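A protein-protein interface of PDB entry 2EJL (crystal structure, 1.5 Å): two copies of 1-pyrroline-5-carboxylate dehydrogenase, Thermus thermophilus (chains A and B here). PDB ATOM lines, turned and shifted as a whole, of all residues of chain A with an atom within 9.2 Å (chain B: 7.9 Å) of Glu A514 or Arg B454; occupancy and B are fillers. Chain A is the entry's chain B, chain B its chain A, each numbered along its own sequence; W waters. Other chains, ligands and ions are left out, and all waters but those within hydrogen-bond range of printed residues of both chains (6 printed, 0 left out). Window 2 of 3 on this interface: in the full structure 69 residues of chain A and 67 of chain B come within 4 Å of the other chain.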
ATOM      1  N   TYR A 162     -19.936 -30.492  24.906  1.00  0.00           N
ATOM      2  CA  TYR A 162     -21.242 -30.936  25.360  1.00  0.00           C
ATOM      3  C   TYR A 162     -22.043 -31.345  24.133  1.00  0.00           C
ATOM      4  O   TYR A 162     -21.935 -30.679  23.102  1.00  0.00           O
ATOM      5  CB  TYR A 162     -21.958 -29.805  26.111  1.00  0.00           C
ATOM      6  CG  TYR A 162     -23.202 -30.272  26.838  1.00  0.00           C
ATOM      7  CD1 TYR A 162     -23.108 -30.917  28.067  1.00  0.00           C
ATOM      8  CD2 TYR A 162     -24.473 -30.093  26.278  1.00  0.00           C
ATOM      9  CE1 TYR A 162     -24.260 -31.368  28.738  1.00  0.00           C
ATOM     10  CE2 TYR A 162     -25.641 -30.537  26.950  1.00  0.00           C
ATOM     11  CZ  TYR A 162     -25.513 -31.171  28.171  1.00  0.00           C
ATOM     12  OH  TYR A 162     -26.634 -31.620  28.837  1.00  0.00           O
ATOM     13  N   PRO A 163     -22.822 -32.441  24.231  1.00  0.00           N
ATOM     14  CA  PRO A 163     -23.628 -32.898  23.088  1.00  0.00           C
ATOM     15  C   PRO A 163     -24.587 -31.846  22.526  1.00  0.00           C
ATOM     16  O   PRO A 163     -25.285 -31.147  23.283  1.00  0.00           O
ATOM     17  CB  PRO A 163     -24.430 -34.083  23.668  1.00  0.00           C
ATOM     18  CG  PRO A 163     -23.653 -34.531  24.824  1.00  0.00           C
ATOM     19  CD  PRO A 163     -23.007 -33.310  25.404  1.00  0.00           C
ATOM     20  N   GLY A 164     -24.604 -31.764  21.204  1.00  0.00           N
ATOM     21  CA  GLY A 164     -25.546 -30.921  20.483  1.00  0.00           C
ATOM     22  C   GLY A 164     -25.277 -29.427  20.570  1.00  0.00           C
ATOM     23  O   GLY A 164     -26.132 -28.622  20.193  1.00  0.00           O
ATOM     24  N   GLU A 165     -24.093 -29.064  21.054  1.00  0.00           N
ATOM     25  CA  GLU A 165     -23.739 -27.649  21.235  1.00  0.00           C
ATOM     26  C   GLU A 165     -22.334 -27.380  20.775  1.00  0.00           C
ATOM     27  O   GLU A 165     -21.475 -28.260  20.849  1.00  0.00           O
ATOM     28  CB  GLU A 165     -23.723 -27.303  22.717  1.00  0.00           C
ATOM     29  CG  GLU A 165     -25.033 -27.325  23.436  1.00  0.00           C
ATOM     30  CD  GLU A 165     -24.957 -26.690  24.819  1.00  0.00           C
ATOM     31  OE1 GLU A 165     -26.028 -26.290  25.299  1.00  0.00           O
ATOM     32  OE2 GLU A 165     -23.863 -26.615  25.446  1.00  0.00           O
ATOM     33  N   ASP A 166     -22.108 -26.150  20.315  1.00  0.00           N
ATOM     34  CA  ASP A 166     -20.781 -25.595  20.228  1.00  0.00           C
ATOM     35  C   ASP A 166     -20.560 -24.755  21.465  1.00  0.00           C
ATOM     36  O   ASP A 166     -21.404 -23.930  21.798  1.00  0.00           O
ATOM     37  CB  ASP A 166     -20.642 -24.682  19.007  1.00  0.00           C
ATOM     38  CG  ASP A 166     -19.266 -24.056  18.914  1.00  0.00           C
ATOM     39  OD1 ASP A 166     -19.158 -22.830  18.712  1.00  0.00           O
ATOM     40  OD2 ASP A 166     -18.287 -24.804  19.062  1.00  0.00           O
ATOM     41  N   ASN A 167     -19.429 -24.949  22.124  1.00  0.00           N
ATOM     42  CA  ASN A 167     -19.066 -24.135  23.267  1.00  0.00           C
ATOM     43  C   ASN A 167     -17.740 -23.483  23.001  1.00  0.00           C
ATOM     44  O   ASN A 167     -16.749 -24.159  22.763  1.00  0.00           O
ATOM     45  CB  ASN A 167     -19.057 -24.967  24.539  1.00  0.00           C
ATOM     46  CG  ASN A 167     -20.440 -25.175  25.069  1.00  0.00           C
ATOM     47  OD1 ASN A 167     -21.014 -24.282  25.714  1.00  0.00           O
ATOM     48  ND2 ASN A 167     -21.004 -26.349  24.789  1.00  0.00           N
ATOM     49  N   GLU A 168     -17.753 -22.155  22.968  1.00  0.00           N
ATOM     50  CA  GLU A 168     -16.590 -21.406  22.519  1.00  0.00           C
ATOM     51  C   GLU A 168     -16.233 -20.331  23.526  1.00  0.00           C
ATOM     52  O   GLU A 168     -16.985 -19.372  23.705  1.00  0.00           O
ATOM     53  CB  GLU A 168     -16.887 -20.767  21.166  1.00  0.00           C
ATOM     54  CG  GLU A 168     -15.710 -20.070  20.553  1.00  0.00           C
ATOM     55  CD  GLU A 168     -16.056 -19.527  19.194  1.00  0.00           C
ATOM     56  OE1 GLU A 168     -16.640 -18.420  19.152  1.00  0.00           O
ATOM     57  OE2 GLU A 168     -15.746 -20.201  18.178  1.00  0.00           O
ATOM     58  N   ALA A 511     -17.663 -16.731  27.277  1.00  0.00           N
ATOM     59  CA  ALA A 511     -18.045 -18.100  26.938  1.00  0.00           C
ATOM     60  C   ALA A 511     -19.367 -18.070  26.200  1.00  0.00           C
ATOM     61  O   ALA A 511     -20.360 -17.597  26.747  1.00  0.00           O
ATOM     62  CB  ALA A 511     -18.145 -18.975  28.203  1.00  0.00           C
ATOM     63  N   VAL A 512     -19.375 -18.581  24.971  1.00  0.00           N
ATOM     64  CA  VAL A 512     -20.564 -18.526  24.120  1.00  0.00           C
ATOM     65  C   VAL A 512     -20.974 -19.932  23.664  1.00  0.00           C
ATOM     66  O   VAL A 512     -20.200 -20.635  23.001  1.00  0.00           O
ATOM     67  CB  VAL A 512     -20.380 -17.575  22.880  1.00  0.00           C
ATOM     68  CG1 VAL A 512     -21.697 -17.447  22.091  1.00  0.00           C
ATOM     69  CG2 VAL A 512     -19.843 -16.208  23.276  1.00  0.00           C
ATOM     70  N   ALA A 513     -22.192 -20.333  24.038  1.00  0.00           N
ATOM     71  CA  ALA A 513     -22.748 -21.644  23.681  1.00  0.00           C
ATOM     72  C   ALA A 513     -23.815 -21.481  22.623  1.00  0.00           C
ATOM     73  O   ALA A 513     -24.667 -20.602  22.762  1.00  0.00           O
ATOM     74  CB  ALA A 513     -23.386 -22.278  24.889  1.00  0.00           C
ATOM     75  N   GLU A 514     -23.818 -22.341  21.603  1.00  0.00           N
ATOM     76  CA  GLU A 514     -24.972 -22.427  20.697  1.00  0.00           C
ATOM     77  C   GLU A 514     -25.541 -23.850  20.702  1.00  0.00           C
ATOM     78  O   GLU A 514     -24.823 -24.814  20.417  1.00  0.00           O
ATOM     79  CB  GLU A 514     -24.632 -22.021  19.265  1.00  0.00           C
ATOM     80  CG  GLU A 514     -25.875 -22.155  18.370  1.00  0.00           C
ATOM     81  CD  GLU A 514     -25.719 -21.691  16.934  1.00  0.00           C
ATOM     82  OE1 GLU A 514     -24.679 -21.098  16.591  1.00  0.00           O
ATOM     83  OE2 GLU A 514     -26.667 -21.930  16.135  1.00  0.00           O
ATOM     84  N   ARG A 515     -26.818 -23.983  21.040  1.00  0.00           N
ATOM     85  CA  ARG A 515     -27.515 -25.254  20.973  1.00  0.00           C
ATOM     86  C   ARG A 515     -28.144 -25.369  19.593  1.00  0.00           C
ATOM     87  O   ARG A 515     -28.992 -24.555  19.223  1.00  0.00           O
ATOM     88  CB  ARG A 515     -28.596 -25.347  22.065  1.00  0.00           C
ATOM     89  CG  ARG A 515     -29.338 -26.701  22.104  1.00  0.00           C
ATOM     90  CD  ARG A 515     -28.520 -27.779  22.794  1.00  0.00           C
ATOM     91  NE  ARG A 515     -28.189 -27.459  24.187  1.00  0.00           N
ATOM     92  CZ  ARG A 515     -29.020 -27.573  25.222  1.00  0.00           C
ATOM     93  NH1 ARG A 515     -30.274 -27.994  25.051  1.00  0.00           N
ATOM     94  NH2 ARG A 515     -28.598 -27.261  26.442  1.00  0.00           N
ATOM     95  N   PHE A 516     -27.720 -26.381  18.836  1.00  0.00           N
ATOM     96  CA  PHE A 516     -28.181 -26.501  17.445  1.00  0.00           C
ATOM     97  C   PHE A 516     -29.561 -27.107  17.290  1.00  0.00           C
ATOM     98  O   PHE A 516     -30.226 -26.851  16.269  1.00  0.00           O
ATOM     99  CB  PHE A 516     -27.168 -27.276  16.606  1.00  0.00           C
ATOM    100  CG  PHE A 516     -25.846 -26.614  16.547  1.00  0.00           C
ATOM    101  CD1 PHE A 516     -24.743 -27.185  17.170  1.00  0.00           C
ATOM    102  CD2 PHE A 516     -25.702 -25.389  15.891  1.00  0.00           C
ATOM    103  CE1 PHE A 516     -23.495 -26.573  17.115  1.00  0.00           C
ATOM    104  CE2 PHE A 516     -24.457 -24.766  15.846  1.00  0.00           C
ATOM    105  CZ  PHE A 516     -23.364 -25.354  16.467  1.00  0.00           C
ATOM    106  OXT PHE A 516     -30.013 -27.852  18.166  1.00  0.00           O
ATOM    107  N   ASP B 298     -35.874 -12.509  18.522  1.00  0.00           N
ATOM    108  CA  ASP B 298     -36.269 -11.802  17.307  1.00  0.00           C
ATOM    109  C   ASP B 298     -37.338 -12.564  16.531  1.00  0.00           C
ATOM    110  O   ASP B 298     -37.759 -13.657  16.933  1.00  0.00           O
ATOM    111  CB  ASP B 298     -35.053 -11.380  16.446  1.00  0.00           C
ATOM    112  CG  ASP B 298     -34.369 -12.532  15.725  1.00  0.00           C
ATOM    113  OD1 ASP B 298     -35.016 -13.562  15.417  1.00  0.00           O
ATOM    114  OD2 ASP B 298     -33.161 -12.343  15.433  1.00  0.00           O
ATOM    115  N   THR B 300     -37.396 -14.183  13.889  1.00  0.00           N
ATOM    116  CA  THR B 300     -36.986 -15.412  13.169  1.00  0.00           C
ATOM    117  C   THR B 300     -36.924 -16.656  14.060  1.00  0.00           C
ATOM    118  O   THR B 300     -36.736 -17.775  13.579  1.00  0.00           O
ATOM    119  CB  THR B 300     -35.589 -15.259  12.495  1.00  0.00           C
ATOM    120  OG1 THR B 300     -34.564 -15.330  13.492  1.00  0.00           O
ATOM    121  CG2 THR B 300     -35.477 -13.944  11.741  1.00  0.00           C
ATOM    122  N   VAL B 449     -29.833 -15.251  23.243  1.00  0.00           N
ATOM    123  CA  VAL B 449     -30.543 -14.853  22.036  1.00  0.00           C
ATOM    124  C   VAL B 449     -31.238 -16.064  21.447  1.00  0.00           C
ATOM    125  O   VAL B 449     -30.588 -17.100  21.230  1.00  0.00           O
ATOM    126  CB  VAL B 449     -29.587 -14.265  20.967  1.00  0.00           C
ATOM    127  CG1 VAL B 449     -30.361 -13.860  19.729  1.00  0.00           C
ATOM    128  CG2 VAL B 449     -28.831 -13.057  21.502  1.00  0.00           C
ATOM    129  N   SER B 451     -32.929 -16.900  17.986  1.00  0.00           N
ATOM    130  CA  SER B 451     -32.920 -16.413  16.609  1.00  0.00           C
ATOM    131  C   SER B 451     -32.446 -17.522  15.676  1.00  0.00           C
ATOM    132  O   SER B 451     -31.598 -18.327  16.043  1.00  0.00           O
ATOM    133  CB  SER B 451     -31.973 -15.215  16.448  1.00  0.00           C
ATOM    134  OG  SER B 451     -31.953 -14.744  15.113  1.00  0.00           O
ATOM    135  N   ARG B 452     -33.023 -17.573  14.478  1.00  0.00           N
ATOM    136  CA  ARG B 452     -32.509 -18.465  13.428  1.00  0.00           C
ATOM    137  C   ARG B 452     -31.562 -17.722  12.481  1.00  0.00           C
ATOM    138  O   ARG B 452     -30.903 -18.340  11.626  1.00  0.00           O
ATOM    139  CB  ARG B 452     -33.651 -19.058  12.611  1.00  0.00           C
ATOM    140  CG  ARG B 452     -34.499 -20.095  13.293  1.00  0.00           C
ATOM    141  CD  ARG B 452     -35.536 -20.596  12.285  1.00  0.00           C
ATOM    142  NE  ARG B 452     -36.394 -21.667  12.787  1.00  0.00           N
ATOM    143  CZ  ARG B 452     -37.597 -21.489  13.327  1.00  0.00           C
ATOM    144  NH1 ARG B 452     -38.308 -22.542  13.732  1.00  0.00           N
ATOM    145  NH2 ARG B 452     -38.101 -20.267  13.474  1.00  0.00           N
ATOM    146  N   LYS B 453     -31.508 -16.394  12.583  1.00  0.00           N
ATOM    147  CA  LYS B 453     -30.662 -15.621  11.680  1.00  0.00           C
ATOM    148  C   LYS B 453     -29.192 -15.662  12.098  1.00  0.00           C
ATOM    149  O   LYS B 453     -28.820 -15.143  13.147  1.00  0.00           O
ATOM    150  CB  LYS B 453     -31.186 -14.189  11.565  1.00  0.00           C
ATOM    151  CG  LYS B 453     -30.474 -13.381  10.516  1.00  0.00           C
ATOM    152  CD  LYS B 453     -31.224 -12.126  10.145  1.00  0.00           C
ATOM    153  CE  LYS B 453     -30.467 -11.384   9.054  1.00  0.00           C
ATOM    154  NZ  LYS B 453     -30.210 -12.237   7.859  1.00  0.00           N
ATOM    155  N   ARG B 454     -28.358 -16.269  11.255  1.00  0.00           N
ATOM    156  CA  ARG B 454     -26.952 -16.457  11.602  1.00  0.00           C
ATOM    157  C   ARG B 454     -26.271 -15.142  11.900  1.00  0.00           C
ATOM    158  O   ARG B 454     -25.423 -15.059  12.784  1.00  0.00           O
ATOM    159  CB  ARG B 454     -26.177 -17.148  10.477  1.00  0.00           C
ATOM    160  CG  ARG B 454     -26.772 -18.468   9.989  1.00  0.00           C
ATOM    161  CD  ARG B 454     -27.027 -19.502  11.091  1.00  0.00           C
ATOM    162  NE  ARG B 454     -25.860 -19.720  11.947  1.00  0.00           N
ATOM    163  CZ  ARG B 454     -25.891 -20.397  13.088  1.00  0.00           C
ATOM    164  NH1 ARG B 454     -24.770 -20.533  13.776  1.00  0.00           N
ATOM    165  NH2 ARG B 454     -27.023 -20.925  13.544  1.00  0.00           N
ATOM    166  N   GLU B 455     -26.618 -14.115  11.132  1.00  0.00           N
ATOM    167  CA  GLU B 455     -25.917 -12.844  11.245  1.00  0.00           C
ATOM    168  C   GLU B 455     -26.247 -12.170  12.571  1.00  0.00           C
ATOM    169  O   GLU B 455     -25.398 -11.480  13.132  1.00  0.00           O
ATOM    170  CB  GLU B 455     -26.253 -11.931  10.076  1.00  0.00           C
ATOM    171  CG  GLU B 455     -25.748 -12.461   8.715  1.00  0.00           C
ATOM    172  CD  GLU B 455     -26.714 -13.420   8.007  1.00  0.00           C
ATOM    173  OE1 GLU B 455     -27.753 -13.851   8.586  1.00  0.00           O
ATOM    174  OE2 GLU B 455     -26.426 -13.735   6.823  1.00  0.00           O
ATOM    175  N   HIS B 456     -27.451 -12.400  13.089  1.00  0.00           N
ATOM    176  CA  HIS B 456     -27.830 -11.886  14.397  1.00  0.00           C
ATOM    177  C   HIS B 456     -27.071 -12.626  15.493  1.00  0.00           C
ATOM    178  O   HIS B 456     -26.548 -12.006  16.418  1.00  0.00           O
ATOM    179  CB  HIS B 456     -29.333 -12.003  14.583  1.00  0.00           C
ATOM    180  CG  HIS B 456     -30.103 -10.998  13.784  1.00  0.00           C
ATOM    181  ND1 HIS B 456     -31.472 -10.875  13.862  1.00  0.00           N
ATOM    182  CD2 HIS B 456     -29.684 -10.046  12.916  1.00  0.00           C
ATOM    183  CE1 HIS B 456     -31.868  -9.904  13.055  1.00  0.00           C
ATOM    184  NE2 HIS B 456     -30.806  -9.387  12.470  1.00  0.00           N
ATOM    185  N   LEU B 457     -26.980 -13.948  15.377  1.00  0.00           N
ATOM    186  CA  LEU B 457     -26.257 -14.735  16.374  1.00  0.00           C
ATOM    187  C   LEU B 457     -24.797 -14.324  16.454  1.00  0.00           C
ATOM    188  O   LEU B 457     -24.243 -14.135  17.537  1.00  0.00           O
ATOM    189  CB  LEU B 457     -26.395 -16.238  16.092  1.00  0.00           C
ATOM    190  CG  LEU B 457     -27.814 -16.819  16.237  1.00  0.00           C
ATOM    191  CD1 LEU B 457     -27.771 -18.303  15.929  1.00  0.00           C
ATOM    192  CD2 LEU B 457     -28.395 -16.556  17.651  1.00  0.00           C
ATOM    193  N   GLU B 458     -24.160 -14.187  15.298  1.00  0.00           N
ATOM    194  CA  GLU B 458     -22.735 -13.910  15.275  1.00  0.00           C
ATOM    195  C   GLU B 458     -22.451 -12.466  15.697  1.00  0.00           C
ATOM    196  O   GLU B 458     -21.423 -12.180  16.342  1.00  0.00           O
ATOM    197  CB  GLU B 458     -22.144 -14.260  13.915  1.00  0.00           C
ATOM    198  CG  GLU B 458     -22.323 -15.746  13.538  1.00  0.00           C
ATOM    199  CD  GLU B 458     -21.663 -16.738  14.494  1.00  0.00           C
ATOM    200  OE1 GLU B 458     -21.877 -17.960  14.303  1.00  0.00           O
ATOM    201  OE2 GLU B 458     -20.930 -16.317  15.411  1.00  0.00           O
ATOM    202  N   TRP B 459     -23.360 -11.563  15.331  1.00  0.00           N
ATOM    203  CA  TRP B 459     -23.361 -10.187  15.841  1.00  0.00           C
ATOM    204  C   TRP B 459     -23.384 -10.180  17.387  1.00  0.00           C
ATOM    205  O   TRP B 459     -22.537  -9.560  18.016  1.00  0.00           O
ATOM    206  CB  TRP B 459     -24.571  -9.466  15.253  1.00  0.00           C
ATOM    207  CG  TRP B 459     -24.718  -8.012  15.510  1.00  0.00           C
ATOM    208  CD1 TRP B 459     -23.875  -7.196  16.186  1.00  0.00           C
ATOM    209  CD2 TRP B 459     -25.795  -7.193  15.043  1.00  0.00           C
ATOM    210  NE1 TRP B 459     -24.366  -5.906  16.186  1.00  0.00           N
ATOM    211  CE2 TRP B 459     -25.540  -5.879  15.478  1.00  0.00           C
ATOM    212  CE3 TRP B 459     -26.946  -7.445  14.279  1.00  0.00           C
ATOM    213  CZ2 TRP B 459     -26.408  -4.812  15.200  1.00  0.00           C
ATOM    214  CZ3 TRP B 459     -27.811  -6.380  13.997  1.00  0.00           C
ATOM    215  CH2 TRP B 459     -27.529  -5.086  14.457  1.00  0.00           C
ATOM    216  N   ALA B 460     -24.333 -10.903  17.984  1.00  0.00           N
ATOM    217  CA  ALA B 460     -24.419 -11.006  19.441  1.00  0.00           C
ATOM    218  C   ALA B 460     -23.141 -11.630  20.021  1.00  0.00           C
ATOM    219  O   ALA B 460     -22.667 -11.214  21.066  1.00  0.00           O
ATOM    220  CB  ALA B 460     -25.632 -11.817  19.857  1.00  0.00           C
ATOM    221  N   ARG B 461     -22.579 -12.640  19.353  1.00  0.00           N
ATOM    222  CA  ARG B 461     -21.300 -13.211  19.812  1.00  0.00           C
ATOM    223  C   ARG B 461     -20.230 -12.130  20.011  1.00  0.00           C
ATOM    224  O   ARG B 461     -19.471 -12.175  20.980  1.00  0.00           O
ATOM    225  CB  ARG B 461     -20.794 -14.264  18.817  1.00  0.00           C
ATOM    226  CG  ARG B 461     -19.503 -15.004  19.219  1.00  0.00           C
ATOM    227  CD  ARG B 461     -19.110 -16.123  18.197  1.00  0.00           C
ATOM    228  NE  ARG B 461     -20.197 -17.089  18.026  1.00  0.00           N
ATOM    229  CZ  ARG B 461     -20.355 -18.186  18.771  1.00  0.00           C
ATOM    230  NH1 ARG B 461     -19.444 -18.522  19.676  1.00  0.00           N
ATOM    231  NH2 ARG B 461     -21.413 -18.966  18.588  1.00  0.00           N
ATOM    232  N   ARG B 462     -20.214 -11.154  19.100  1.00  0.00           N
ATOM    233  CA  ARG B 462     -19.238 -10.062  19.101  1.00  0.00           C
ATOM    234  C   ARG B 462     -19.619  -8.923  20.054  1.00  0.00           C
ATOM    235  O   ARG B 462     -18.733  -8.282  20.617  1.00  0.00           O
ATOM    236  CB  ARG B 462     -19.042  -9.509  17.676  1.00  0.00           C
ATOM    237  CG  ARG B 462     -18.593 -10.560  16.622  1.00  0.00           C
ATOM    238  CD  ARG B 462     -18.377  -9.969  15.199  1.00  0.00           C
ATOM    239  NE  ARG B 462     -19.458  -9.079  14.754  1.00  0.00           N
ATOM    240  CZ  ARG B 462     -20.428  -9.404  13.901  1.00  0.00           C
ATOM    241  NH1 ARG B 462     -20.493 -10.621  13.353  1.00  0.00           N
ATOM    242  NH2 ARG B 462     -21.348  -8.494  13.593  1.00  0.00           N
ATOM    243  N   LEU B 469     -22.825 -16.225  27.358  1.00  0.00           N
ATOM    244  CA  LEU B 469     -23.849 -15.981  26.364  1.00  0.00           C
ATOM    245  C   LEU B 469     -24.340 -17.305  25.762  1.00  0.00           C
ATOM    246  O   LEU B 469     -23.534 -18.175  25.444  1.00  0.00           O
ATOM    247  CB  LEU B 469     -23.267 -15.064  25.280  1.00  0.00           C
ATOM    248  CG  LEU B 469     -24.148 -14.629  24.104  1.00  0.00           C
ATOM    249  CD1 LEU B 469     -25.425 -13.866  24.559  1.00  0.00           C
ATOM    250  CD2 LEU B 469     -23.298 -13.825  23.133  1.00  0.00           C
ATOM    251  N   TYR B 470     -25.653 -17.457  25.604  1.00  0.00           N
ATOM    252  CA  TYR B 470     -26.245 -18.715  25.116  1.00  0.00           C
ATOM    253  C   TYR B 470     -27.216 -18.447  23.980  1.00  0.00           C
ATOM    254  O   TYR B 470     -28.046 -17.530  24.073  1.00  0.00           O
ATOM    255  CB  TYR B 470     -26.998 -19.404  26.241  1.00  0.00           C
ATOM    256  CG  TYR B 470     -26.143 -19.661  27.456  1.00  0.00           C
ATOM    257  CD1 TYR B 470     -26.029 -18.686  28.469  1.00  0.00           C
ATOM    258  CD2 TYR B 470     -25.467 -20.876  27.613  1.00  0.00           C
ATOM    259  CE1 TYR B 470     -25.238 -18.919  29.604  1.00  0.00           C
ATOM    260  CE2 TYR B 470     -24.696 -21.126  28.733  1.00  0.00           C
ATOM    261  CZ  TYR B 470     -24.575 -20.138  29.729  1.00  0.00           C
ATOM    262  OH  TYR B 470     -23.800 -20.335  30.849  1.00  0.00           O
ATOM    263  N   PHE B 471     -27.136 -19.268  22.929  1.00  0.00           N
ATOM    264  CA  PHE B 471     -27.993 -19.103  21.758  1.00  0.00           C
ATOM    265  C   PHE B 471     -28.962 -20.271  21.657  1.00  0.00           C
ATOM    266  O   PHE B 471     -28.542 -21.448  21.652  1.00  0.00           O
ATOM    267  CB  PHE B 471     -27.176 -19.005  20.465  1.00  0.00           C
ATOM    268  CG  PHE B 471     -26.270 -17.802  20.387  1.00  0.00           C
ATOM    269  CD1 PHE B 471     -26.563 -16.619  21.078  1.00  0.00           C
ATOM    270  CD2 PHE B 471     -25.118 -17.843  19.591  1.00  0.00           C
ATOM    271  CE1 PHE B 471     -25.704 -15.512  21.004  1.00  0.00           C
ATOM    272  CE2 PHE B 471     -24.266 -16.743  19.507  1.00  0.00           C
ATOM    273  CZ  PHE B 471     -24.564 -15.559  20.215  1.00  0.00           C
ATOM    274  N   ASN B 472     -30.251 -19.942  21.599  1.00  0.00           N
ATOM    275  CA  ASN B 472     -31.327 -20.919  21.388  1.00  0.00           C
ATOM    276  C   ASN B 472     -31.422 -22.000  22.463  1.00  0.00           C
ATOM    277  O   ASN B 472     -31.743 -23.164  22.187  1.00  0.00           O
ATOM    278  CB  ASN B 472     -31.241 -21.514  19.976  1.00  0.00           C
ATOM    279  CG  ASN B 472     -31.517 -20.467  18.897  1.00  0.00           C
ATOM    280  OD1 ASN B 472     -32.423 -19.648  19.057  1.00  0.00           O
ATOM    281  ND2 ASN B 472     -30.710 -20.457  17.821  1.00  0.00           N
ATOM    282  N   ARG B 473     -31.192 -21.560  23.695  1.00  0.00           N
ATOM    283  CA  ARG B 473     -31.286 -22.404  24.872  1.00  0.00           C
ATOM    284  C   ARG B 473     -31.332 -21.530  26.116  1.00  0.00           C
ATOM    285  O   ARG B 473     -31.076 -20.330  26.056  1.00  0.00           O
ATOM    286  CB  ARG B 473     -30.093 -23.379  24.983  1.00  0.00           C
ATOM    287  CG  ARG B 473     -28.715 -22.710  24.947  1.00  0.00           C
ATOM    288  CD  ARG B 473     -27.689 -23.555  25.686  1.00  0.00           C
ATOM    289  NE  ARG B 473     -27.813 -23.318  27.124  1.00  0.00           N
ATOM    290  CZ  ARG B 473     -27.121 -23.942  28.067  1.00  0.00           C
ATOM    291  NH1 ARG B 473     -26.240 -24.899  27.741  1.00  0.00           N
ATOM    292  NH2 ARG B 473     -27.329 -23.617  29.337  1.00  0.00           N
ATOM    293  N   GLN B 483     -18.692 -24.441  30.191  1.00  0.00           N
ATOM    294  CA  GLN B 483     -18.964 -23.002  30.139  1.00  0.00           C
ATOM    295  C   GLN B 483     -18.311 -22.281  31.318  1.00  0.00           C
ATOM    296  O   GLN B 483     -18.943 -22.126  32.364  1.00  0.00           O
ATOM    297  CB  GLN B 483     -20.483 -22.795  30.149  1.00  0.00           C
ATOM    298  CG  GLN B 483     -21.119 -23.286  28.864  1.00  0.00           C
ATOM    299  CD  GLN B 483     -22.232 -24.328  29.066  1.00  0.00           C
ATOM    300  OE1 GLN B 483     -22.652 -24.638  30.189  1.00  0.00           O
ATOM    301  NE2 GLN B 483     -22.701 -24.888  27.949  1.00  0.00           N
HETATM  302  O   HOH W   1     -28.997 -22.692  17.262  1.00  0.00           O
HETATM  303  O   HOH W   2     -21.672 -19.870  27.716  1.00  0.00           O
HETATM  304  O   HOH W   3     -31.584 -24.921  20.196  1.00  0.00           O
HETATM  305  O   HOH W   4     -20.656 -21.151  20.222  1.00  0.00           O
HETATM  306  O   HOH W   5     -23.523 -18.682  16.564  1.00  0.00           O
HETATM  307  O   HOH W   6     -24.488 -27.202  28.000  1.00  0.00           O
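Printed residues of chain B within 4 Å of Glu A165: Arg B473 and Gln B483. Of the printed residues of chain B, Glu A514 touches Arg B454, Leu B457 and Phe B471. Arg B454 touches one residue of chain A. No residue of chain A comes within 4 Å of Glu B455. Of the printed residues of chain A, Asn B472 touches Arg A515. The nearest residue of chain B that does not touch Glu A514 is Arg B461 (4.4 Å). The nearest residue of chain A that does not touch Arg B454 is Phe A516 (4.7 Å).
The backbone carbonyl oxygen (O) of Ser B451 is in hydrogen-bond range of the side-chain amide nitrogen (ND2) of Asn B472 (2.9 Å). The guanidinium group (NH1) of Arg B454 is in salt-bridge range of the side-chain carboxylate (OE1) of Glu B458 (3.9 Å).
Water W3 bridges O of Asn B472 (2.7 Å) and O of Arg A515 (2.8 Å). Water W4 lies within hydrogen-bond range of the side-chain carboxylate of Asp A166 (2.7 Å), the guanidinium group of Arg B461 (2.8 Å) and the backbone carbonyl oxygen of Val A512 (2.9 Å).
No position is printed for both chains. Of the 17 pairs that touch across the chains among the printed residues, none has its exchanged pair printed and touching as well.
Val A512 touches Arg B461. CA of Val A512 touches O of Leu B469, at 3.3 Å. Phe B471 touches Val A512 (CE2 to CG1, 3.7 Å). Ala A513 touches Tyr B470 (O to CA, 3.4 Å). CD1 of Leu B457 touches OE2 of Glu A514 (3.8 Å). CA of Glu A514 touches O of Phe B471, 3.8 Å away. Asn B472 touches Arg A515 (O to CB, 3.8 Å). NH1 of Arg B473 touches NH2 of Arg A515, 3.6 Å away.
The guanidinium group of Arg B461 is in salt-bridge range of the side-chain carboxylate of Glu A168, 2.9 Å away. The guanidinium group of Arg B473 lies within salt-bridge range of the side-chain carboxylate of Glu A165 (2.8 Å). The side-chain carboxylate (OE2) of Glu A514 lies within salt-bridge range of the guanidinium group (NH2) of Arg B454, at 2.8 Å. The backbone carbonyl oxygen of Ala A513 is in hydrogen-bond range of the backbone NH of Phe B471 (2.8 Å). The backbone carbonyl oxygen (O) of Leu B469 is in hydrogen-bond range of the backbone NH (N) of Ala A513 (2.9 Å). The backbone NH of Arg A515 is in hydrogen-bond range of the backbone carbonyl oxygen of Phe B471 (3.1 Å). O of Ala A511 sits at hydrogen-bond distance from N of Leu B469, at 2.9 Å. The side-chain amide oxygen (OD1) of Asn A167 is in hydrogen-bond range of the side-chain amide nitrogen (NE2) of Gln B483 (2.9 Å). The side-chain amide nitrogen (NE2) of Gln B483 is in hydrogen-bond range of the side-chain carboxylate (OE2) of Glu A165, 3.3 Å away.
Of the 21 printed residues of chain B, 9 touch a printed residue of chain A. Printed residues of chain B that touch a printed residue of chain A: Arg B454, Leu B457, Arg B461, Leu B469, Tyr B470, Phe B471, Asn B472, Arg B473 and Gln B483. Hydrophobic or aromatic side chains of chain B that line the printed part of chain A: Leu B457, Tyr B470 and Phe B471. Of the 13 printed residues of chain A, 8 touch a printed residue of chain B. Among the printed residues, Asp or Glu carboxylates within 4 Å of a Lys or Arg side-chain nitrogen of the other chain: Glu A165 with Arg B473, Glu A168 with Arg B461 and Glu A514 with Arg B454.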
